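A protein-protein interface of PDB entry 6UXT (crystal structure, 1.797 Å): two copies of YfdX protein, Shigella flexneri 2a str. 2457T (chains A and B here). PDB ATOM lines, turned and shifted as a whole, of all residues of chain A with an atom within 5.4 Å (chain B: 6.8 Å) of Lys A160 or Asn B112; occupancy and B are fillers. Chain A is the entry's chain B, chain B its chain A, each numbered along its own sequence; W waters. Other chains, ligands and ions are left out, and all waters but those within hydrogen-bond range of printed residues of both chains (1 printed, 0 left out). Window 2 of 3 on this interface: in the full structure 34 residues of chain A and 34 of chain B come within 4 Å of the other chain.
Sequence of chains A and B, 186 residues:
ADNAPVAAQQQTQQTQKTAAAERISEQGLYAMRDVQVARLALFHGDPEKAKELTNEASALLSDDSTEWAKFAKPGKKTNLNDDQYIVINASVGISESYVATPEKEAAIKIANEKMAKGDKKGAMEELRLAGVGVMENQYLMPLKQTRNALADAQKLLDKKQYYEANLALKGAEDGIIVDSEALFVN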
ATOM      1  N   GLU A  48     -16.224   9.542  -4.217  1.00  0.00           N
ATOM      2  CA  GLU A  48     -17.616   9.170  -4.457  1.00  0.00           C
ATOM      3  C   GLU A  48     -18.341  10.244  -5.258  1.00  0.00           C
ATOM      4  O   GLU A  48     -19.148   9.928  -6.144  1.00  0.00           O
ATOM      5  CB  GLU A  48     -18.330   8.896  -3.132  1.00  0.00           C
ATOM      6  CG  GLU A  48     -17.791   7.663  -2.406  1.00  0.00           C
ATOM      7  CD  GLU A  48     -17.576   6.477  -3.341  1.00  0.00           C
ATOM      8  OE1 GLU A  48     -18.532   6.086  -4.050  1.00  0.00           O
ATOM      9  OE2 GLU A  48     -16.444   5.946  -3.382  1.00  0.00           O
ATOM     10  N   LYS A  51     -17.166   9.970  -8.852  1.00  0.00           N
ATOM     11  CA  LYS A  51     -17.832   8.860  -9.525  1.00  0.00           C
ATOM     12  C   LYS A  51     -19.248   9.239  -9.939  1.00  0.00           C
ATOM     13  O   LYS A  51     -19.689   8.911 -11.046  1.00  0.00           O
ATOM     14  CB  LYS A  51     -17.870   7.626  -8.612  1.00  0.00           C
ATOM     15  CG  LYS A  51     -16.544   6.900  -8.459  1.00  0.00           C
ATOM     16  CD  LYS A  51     -16.608   5.869  -7.341  1.00  0.00           C
ATOM     17  CE  LYS A  51     -15.208   5.519  -6.843  1.00  0.00           C
ATOM     18  NZ  LYS A  51     -15.242   4.961  -5.458  1.00  0.00           N
ATOM     19  N   LEU A 156     -11.352   2.857 -14.790  1.00  0.00           N
ATOM     20  CA  LEU A 156     -10.334   3.174 -13.796  1.00  0.00           C
ATOM     21  C   LEU A 156     -10.963   3.485 -12.444  1.00  0.00           C
ATOM     22  O   LEU A 156     -10.483   3.003 -11.406  1.00  0.00           O
ATOM     23  CB  LEU A 156      -9.473   4.340 -14.294  1.00  0.00           C
ATOM     24  CG  LEU A 156      -8.645   3.977 -15.523  1.00  0.00           C
ATOM     25  CD1 LEU A 156      -8.198   5.246 -16.232  1.00  0.00           C
ATOM     26  CD2 LEU A 156      -7.424   3.122 -15.148  1.00  0.00           C
ATOM     27  N   LEU A 157     -12.048   4.271 -12.436  1.00  0.00           N
ATOM     28  CA  LEU A 157     -12.721   4.577 -11.176  1.00  0.00           C
ATOM     29  C   LEU A 157     -13.228   3.311 -10.502  1.00  0.00           C
ATOM     30  O   LEU A 157     -13.199   3.203  -9.270  1.00  0.00           O
ATOM     31  CB  LEU A 157     -13.881   5.547 -11.405  1.00  0.00           C
ATOM     32  CG  LEU A 157     -13.520   6.991 -11.766  1.00  0.00           C
ATOM     33  CD1 LEU A 157     -14.785   7.726 -12.267  1.00  0.00           C
ATOM     34  CD2 LEU A 157     -12.927   7.702 -10.567  1.00  0.00           C
ATOM     35  N   ASP A 158     -13.693   2.340 -11.294  1.00  0.00           N
ATOM     36  CA  ASP A 158     -14.191   1.092 -10.715  1.00  0.00           C
ATOM     37  C   ASP A 158     -13.076   0.288 -10.064  1.00  0.00           C
ATOM     38  O   ASP A 158     -13.336  -0.489  -9.141  1.00  0.00           O
ATOM     39  CB  ASP A 158     -14.879   0.238 -11.781  1.00  0.00           C
ATOM     40  CG  ASP A 158     -16.226   0.789 -12.177  1.00  0.00           C
ATOM     41  OD1 ASP A 158     -16.764   1.621 -11.414  1.00  0.00           O
ATOM     42  OD2 ASP A 158     -16.740   0.393 -13.248  1.00  0.00           O
ATOM     43  N   LYS A 159     -11.845   0.441 -10.536  1.00  0.00           N
ATOM     44  CA  LYS A 159     -10.691  -0.230  -9.955  1.00  0.00           C
ATOM     45  C   LYS A 159      -9.983   0.610  -8.899  1.00  0.00           C
ATOM     46  O   LYS A 159      -8.909   0.210  -8.428  1.00  0.00           O
ATOM     47  CB  LYS A 159      -9.698  -0.618 -11.053  1.00  0.00           C
ATOM     48  CG  LYS A 159     -10.215  -1.695 -11.992  1.00  0.00           C
ATOM     49  CD  LYS A 159      -9.257  -1.924 -13.145  1.00  0.00           C
ATOM     50  CE  LYS A 159      -9.861  -2.852 -14.190  1.00  0.00           C
ATOM     51  NZ  LYS A 159     -10.200  -4.192 -13.625  1.00  0.00           N
ATOM     52  N   LYS A 160     -10.559   1.749  -8.515  1.00  0.00           N
ATOM     53  CA  LYS A 160      -9.998   2.643  -7.504  1.00  0.00           C
ATOM     54  C   LYS A 160      -8.673   3.250  -7.959  1.00  0.00           C
ATOM     55  O   LYS A 160      -7.831   3.613  -7.133  1.00  0.00           O
ATOM     56  CB  LYS A 160      -9.829   1.930  -6.153  1.00  0.00           C
ATOM     57  CG  LYS A 160     -11.011   1.040  -5.765  1.00  0.00           C
ATOM     58  CD  LYS A 160     -12.091   1.824  -5.038  1.00  0.00           C
ATOM     59  CE  LYS A 160     -11.610   2.272  -3.655  1.00  0.00           C
ATOM     60  NZ  LYS A 160     -12.464   3.358  -3.062  1.00  0.00           N
ATOM     61  N   GLN A 161      -8.478   3.353  -9.277  1.00  0.00           N
ATOM     62  CA  GLN A 161      -7.268   3.950  -9.842  1.00  0.00           C
ATOM     63  C   GLN A 161      -7.531   5.434 -10.079  1.00  0.00           C
ATOM     64  O   GLN A 161      -7.734   5.897 -11.207  1.00  0.00           O
ATOM     65  CB  GLN A 161      -6.871   3.236 -11.126  1.00  0.00           C
ATOM     66  CG  GLN A 161      -6.328   1.829 -10.914  1.00  0.00           C
ATOM     67  CD  GLN A 161      -5.980   1.171 -12.225  1.00  0.00           C
ATOM     68  OE1 GLN A 161      -6.752   0.371 -12.750  1.00  0.00           O
ATOM     69  NE2 GLN A 161      -4.822   1.531 -12.782  1.00  0.00           N
ATOM     70  N   TYR A 162      -7.519   6.191  -8.980  1.00  0.00           N
ATOM     71  CA  TYR A 162      -8.046   7.556  -9.006  1.00  0.00           C
ATOM     72  C   TYR A 162      -7.129   8.523  -9.747  1.00  0.00           C
ATOM     73  O   TYR A 162      -7.611   9.382 -10.491  1.00  0.00           O
ATOM     74  CB  TYR A 162      -8.290   8.026  -7.584  1.00  0.00           C
ATOM     75  CG  TYR A 162      -9.365   7.195  -6.926  1.00  0.00           C
ATOM     76  CD1 TYR A 162     -10.574   6.989  -7.572  1.00  0.00           C
ATOM     77  CD2 TYR A 162      -9.163   6.592  -5.681  1.00  0.00           C
ATOM     78  CE1 TYR A 162     -11.573   6.223  -6.998  1.00  0.00           C
ATOM     79  CE2 TYR A 162     -10.163   5.813  -5.095  1.00  0.00           C
ATOM     80  CZ  TYR A 162     -11.368   5.641  -5.765  1.00  0.00           C
ATOM     81  OH  TYR A 162     -12.399   4.884  -5.234  1.00  0.00           O
ATOM     82  N   TYR A 163      -5.810   8.430  -9.545  1.00  0.00           N
ATOM     83  CA  TYR A 163      -4.919   9.312 -10.302  1.00  0.00           C
ATOM     84  C   TYR A 163      -5.042   9.049 -11.800  1.00  0.00           C
ATOM     85  O   TYR A 163      -5.142   9.986 -12.605  1.00  0.00           O
ATOM     86  CB  TYR A 163      -3.466   9.145  -9.841  1.00  0.00           C
ATOM     87  CG  TYR A 163      -2.499   9.947 -10.694  1.00  0.00           C
ATOM     88  CD1 TYR A 163      -2.425  11.336 -10.576  1.00  0.00           C
ATOM     89  CD2 TYR A 163      -1.704   9.325 -11.650  1.00  0.00           C
ATOM     90  CE1 TYR A 163      -1.562  12.086 -11.396  1.00  0.00           C
ATOM     91  CE2 TYR A 163      -0.843  10.063 -12.467  1.00  0.00           C
ATOM     92  CZ  TYR A 163      -0.778  11.439 -12.328  1.00  0.00           C
ATOM     93  OH  TYR A 163       0.074  12.173 -13.136  1.00  0.00           O
ATOM     94  N   GLU A 164      -5.045   7.770 -12.187  1.00  0.00           N
ATOM     95  CA  GLU A 164      -5.187   7.413 -13.597  1.00  0.00           C
ATOM     96  C   GLU A 164      -6.526   7.890 -14.157  1.00  0.00           C
ATOM     97  O   GLU A 164      -6.602   8.336 -15.307  1.00  0.00           O
ATOM     98  CB  GLU A 164      -5.061   5.894 -13.772  1.00  0.00           C
ATOM     99  CG  GLU A 164      -3.722   5.297 -13.302  1.00  0.00           C
ATOM    100  CD  GLU A 164      -3.758   4.793 -11.851  1.00  0.00           C
ATOM    101  OE1 GLU A 164      -4.346   5.486 -10.990  1.00  0.00           O
ATOM    102  OE2 GLU A 164      -3.198   3.701 -11.577  1.00  0.00           O
ATOM    103  N   ALA B 107       4.291   4.661  -6.081  1.00  0.00           N
ATOM    104  CA  ALA B 107       3.812   5.913  -5.503  1.00  0.00           C
ATOM    105  C   ALA B 107       2.363   6.194  -5.896  1.00  0.00           C
ATOM    106  O   ALA B 107       1.571   6.652  -5.070  1.00  0.00           O
ATOM    107  CB  ALA B 107       4.715   7.075  -5.925  1.00  0.00           C
ATOM    108  N   ILE B 108       2.002   5.942  -7.155  1.00  0.00           N
ATOM    109  CA  ILE B 108       0.622   6.190  -7.582  1.00  0.00           C
ATOM    110  C   ILE B 108      -0.346   5.284  -6.830  1.00  0.00           C
ATOM    111  O   ILE B 108      -1.428   5.716  -6.409  1.00  0.00           O
ATOM    112  CB  ILE B 108       0.496   6.019  -9.107  1.00  0.00           C
ATOM    113  CG1 ILE B 108       1.228   7.167  -9.823  1.00  0.00           C
ATOM    114  CG2 ILE B 108      -0.980   5.935  -9.522  1.00  0.00           C
ATOM    115  CD1 ILE B 108       1.488   6.921 -11.298  1.00  0.00           C
ATOM    116  N   LYS B 109       0.017   4.008  -6.668  1.00  0.00           N
ATOM    117  CA  LYS B 109      -0.818   3.083  -5.909  1.00  0.00           C
ATOM    118  C   LYS B 109      -1.028   3.572  -4.479  1.00  0.00           C
ATOM    119  O   LYS B 109      -2.144   3.510  -3.952  1.00  0.00           O
ATOM    120  CB  LYS B 109      -0.186   1.688  -5.926  1.00  0.00           C
ATOM    121  CG  LYS B 109      -0.924   0.615  -5.131  1.00  0.00           C
ATOM    122  CD  LYS B 109      -0.293  -0.751  -5.396  1.00  0.00           C
ATOM    123  CE  LYS B 109      -0.874  -1.846  -4.503  1.00  0.00           C
ATOM    124  NZ  LYS B 109      -2.286  -2.175  -4.832  1.00  0.00           N
ATOM    125  N   ILE B 110       0.032   4.060  -3.833  1.00  0.00           N
ATOM    126  CA  ILE B 110      -0.113   4.583  -2.478  1.00  0.00           C
ATOM    127  C   ILE B 110      -1.001   5.821  -2.478  1.00  0.00           C
ATOM    128  O   ILE B 110      -1.894   5.958  -1.636  1.00  0.00           O
ATOM    129  CB  ILE B 110       1.270   4.878  -1.861  1.00  0.00           C
ATOM    130  CG1 ILE B 110       2.014   3.577  -1.564  1.00  0.00           C
ATOM    131  CG2 ILE B 110       1.133   5.737  -0.587  1.00  0.00           C
ATOM    132  CD1 ILE B 110       3.517   3.794  -1.317  1.00  0.00           C
ATOM    133  N   ALA B 111      -0.763   6.744  -3.419  1.00  0.00           N
ATOM    134  CA  ALA B 111      -1.589   7.946  -3.507  1.00  0.00           C
ATOM    135  C   ALA B 111      -3.065   7.599  -3.676  1.00  0.00           C
ATOM    136  O   ALA B 111      -3.932   8.249  -3.082  1.00  0.00           O
ATOM    137  CB  ALA B 111      -1.135   8.825  -4.678  1.00  0.00           C
ATOM    138  N   ASN B 112      -3.368   6.600  -4.511  1.00  0.00           N
ATOM    139  CA  ASN B 112      -4.759   6.209  -4.724  1.00  0.00           C
ATOM    140  C   ASN B 112      -5.384   5.686  -3.439  1.00  0.00           C
ATOM    141  O   ASN B 112      -6.559   5.956  -3.153  1.00  0.00           O
ATOM    142  CB  ASN B 112      -4.849   5.132  -5.802  1.00  0.00           C
ATOM    143  CG  ASN B 112      -4.648   5.693  -7.193  1.00  0.00           C
ATOM    144  OD1 ASN B 112      -4.834   6.885  -7.413  1.00  0.00           O
ATOM    145  ND2 ASN B 112      -4.282   4.834  -8.136  1.00  0.00           N
ATOM    146  N   GLU B 113      -4.622   4.902  -2.678  1.00  0.00           N
ATOM    147  CA  GLU B 113      -5.122   4.405  -1.397  1.00  0.00           C
ATOM    148  C   GLU B 113      -5.408   5.557  -0.446  1.00  0.00           C
ATOM    149  O   GLU B 113      -6.435   5.561   0.245  1.00  0.00           O
ATOM    150  CB  GLU B 113      -4.120   3.423  -0.789  1.00  0.00           C
ATOM    151  CG  GLU B 113      -4.111   2.074  -1.473  1.00  0.00           C
ATOM    152  CD  GLU B 113      -2.870   1.252  -1.156  1.00  0.00           C
ATOM    153  OE1 GLU B 113      -1.780   1.844  -0.994  1.00  0.00           O
ATOM    154  OE2 GLU B 113      -2.982   0.011  -1.084  1.00  0.00           O
ATOM    155  N   LYS B 114      -4.531   6.566  -0.424  1.00  0.00           N
ATOM    156  CA  LYS B 114      -4.790   7.750   0.396  1.00  0.00           C
ATOM    157  C   LYS B 114      -6.034   8.498  -0.072  1.00  0.00           C
ATOM    158  O   LYS B 114      -6.824   8.970   0.755  1.00  0.00           O
ATOM    159  CB  LYS B 114      -3.571   8.674   0.397  1.00  0.00           C
ATOM    160  CG  LYS B 114      -2.352   8.073   1.134  1.00  0.00           C
ATOM    161  CD  LYS B 114      -1.182   9.038   1.144  1.00  0.00           C
ATOM    162  CE  LYS B 114       0.032   8.462   1.897  1.00  0.00           C
ATOM    163  NZ  LYS B 114      -0.284   8.163   3.326  1.00  0.00           N
ATOM    164  N   MET B 115      -6.227   8.632  -1.394  1.00  0.00           N
ATOM    165  CA  MET B 115      -7.432   9.291  -1.888  1.00  0.00           C
ATOM    166  C   MET B 115      -8.686   8.525  -1.486  1.00  0.00           C
ATOM    167  O   MET B 115      -9.717   9.130  -1.176  1.00  0.00           O
ATOM    168  CB  MET B 115      -7.379   9.451  -3.406  1.00  0.00           C
ATOM    169  CG  MET B 115      -6.479  10.572  -3.841  1.00  0.00           C
ATOM    170  SD  MET B 115      -6.491  10.780  -5.631  1.00  0.00           S
ATOM    171  CE  MET B 115      -4.969   9.958  -6.086  1.00  0.00           C
ATOM    172  N   ALA B 116      -8.620   7.194  -1.508  1.00  0.00           N
ATOM    173  CA  ALA B 116      -9.784   6.394  -1.145  1.00  0.00           C
ATOM    174  C   ALA B 116     -10.194   6.635   0.300  1.00  0.00           C
ATOM    175  O   ALA B 116     -11.387   6.575   0.626  1.00  0.00           O
ATOM    176  CB  ALA B 116      -9.496   4.911  -1.390  1.00  0.00           C
ATOM    177  N   LYS B 117      -9.231   6.923   1.174  1.00  0.00           N
ATOM    178  CA  LYS B 117      -9.485   7.174   2.590  1.00  0.00           C
ATOM    179  C   LYS B 117      -9.818   8.630   2.870  1.00  0.00           C
ATOM    180  O   LYS B 117     -10.050   8.984   4.032  1.00  0.00           O
ATOM    181  CB  LYS B 117      -8.267   6.774   3.441  1.00  0.00           C
ATOM    182  CG  LYS B 117      -7.748   5.369   3.216  1.00  0.00           C
ATOM    183  CD  LYS B 117      -6.370   5.202   3.869  1.00  0.00           C
ATOM    184  CE  LYS B 117      -6.437   4.376   5.141  1.00  0.00           C
ATOM    185  NZ  LYS B 117      -6.826   2.964   4.864  1.00  0.00           N
ATOM    186  N   ALA B 123      -2.121  12.266  -0.280  1.00  0.00           N
ATOM    187  CA  ALA B 123      -2.117  11.777  -1.654  1.00  0.00           C
ATOM    188  C   ALA B 123      -1.323  12.708  -2.558  1.00  0.00           C
ATOM    189  O   ALA B 123      -0.517  12.255  -3.386  1.00  0.00           O
ATOM    190  CB  ALA B 123      -3.550  11.620  -2.176  1.00  0.00           C
ATOM    191  N   GLU B 126       2.438  12.430  -1.896  1.00  0.00           N
ATOM    192  CA  GLU B 126       2.985  11.205  -2.467  1.00  0.00           C
ATOM    193  C   GLU B 126       3.231  11.360  -3.965  1.00  0.00           C
ATOM    194  O   GLU B 126       4.265  10.913  -4.482  1.00  0.00           O
ATOM    195  CB  GLU B 126       2.028  10.041  -2.186  1.00  0.00           C
ATOM    196  CG  GLU B 126       2.548   8.668  -2.614  1.00  0.00           C
ATOM    197  CD  GLU B 126       3.578   8.063  -1.654  1.00  0.00           C
ATOM    198  OE1 GLU B 126       3.607   8.443  -0.463  1.00  0.00           O
ATOM    199  OE2 GLU B 126       4.352   7.190  -2.104  1.00  0.00           O
ATOM    200  N   LEU B 127       2.282  11.983  -4.681  1.00  0.00           N
ATOM    201  CA  LEU B 127       2.468  12.238  -6.110  1.00  0.00           C
ATOM    202  C   LEU B 127       3.651  13.170  -6.363  1.00  0.00           C
ATOM    203  O   LEU B 127       4.457  12.931  -7.266  1.00  0.00           O
ATOM    204  CB  LEU B 127       1.187  12.826  -6.703  1.00  0.00           C
ATOM    205  CG  LEU B 127       0.015  11.852  -6.761  1.00  0.00           C
ATOM    206  CD1 LEU B 127      -1.270  12.553  -7.278  1.00  0.00           C
ATOM    207  CD2 LEU B 127       0.351  10.633  -7.621  1.00  0.00           C
HETATM  208  O   HOH W   1      -2.635   2.345  -9.285  1.00  0.00           O
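Of chain B, only Asn B112 (3.6 Å) and Ala B116 (3.7 Å) come within 4 Å of Lys A160.
Of the printed residues of chain B, Tyr A163 touches Asn B112 (2.8 Å), Met B115 (3.9 Å) and Leu B127 (3.7 Å).
Asn B112 touches just these residues of chain A: Lys A160, Gln A161, Tyr A162, Tyr A163 and Glu A164.
Glu B113 touches none of the printed residues of chain A.
Of the printed residues of chain A, Met B115 touches Tyr A162 and Tyr A163.
Of the printed residues of chain A, Ala B116 touches Lys A160 (3.7 Å) and Tyr A162 (3.9 Å).
Ala B123 touches none of the printed residues of chain A.
The backbone NH (N) of Tyr A162 lies within hydrogen-bond range of the side-chain amide oxygen (OD1) of Asn B112 (3.2 Å).
The side-chain amide oxygen (OD1) of Asn B112 lies within hydrogen-bond range of the backbone NH (N) of Tyr A163 (2.8 Å).
The side-chain carboxylate of Glu A164 is in hydrogen-bond range of the side-chain amide nitrogen of Asn B112.
The backbone carbonyl oxygen of Ile B108 lies close to the side-chain amide nitrogen of Asn B112, at 3.5 Å.
OH of Tyr A162 lies within hydrogen-bond range of NZ of Lys A51, at 2.9 Å.
The backbone carbonyl oxygen of Leu A156 sits at hydrogen-bond distance from the backbone NH of Gln A161, 2.9 Å away.
The side-chain amino group of Lys A160 lies within hydrogen-bond range of the side-chain hydroxyl of Tyr A162 (2.7 Å).
OE2 of Glu A164 sits at hydrogen-bond distance from NE2 of Gln A161 (3.0 Å).
No position is printed for both chains.
Of the 11 pairs that touch across the chains among the printed residues, none has its exchanged pair printed and touching as well.
Asn B112 touches Lys A160 (CB to O, 3.6 Å).
Ala B116 touches Lys A160.
Gln A161 touches Asn B112.
Met B115 touches Tyr A162.
Ala B116 touches Tyr A162 (CB to CE2, 3.9 Å).
Tyr A163 touches Met B115 (N to CE, 3.9 Å).
Tyr A163 touches Leu B127 (CD1 to CD1, 3.7 Å).
Glu A164 touches Ile B108.
Of the 11 printed residues of chain A, 5 touch a printed residue of chain B.
Printed residues of chain A that touch a printed residue of chain B: Lys A160, Gln A161, Tyr A162, Tyr A163 and Glu A164.
Hydrophobic or aromatic side chains of chain B that line the printed part of chain A: Ile B108, Met B115, Ala B116 and Leu B127.
Among the printed residues, 11 pairs touch across the chains.
Water W1 lies within hydrogen-bond range of the side-chain carboxylate (OE2) of Glu A164 and the side-chain amide nitrogen (ND2) of Asn B112.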
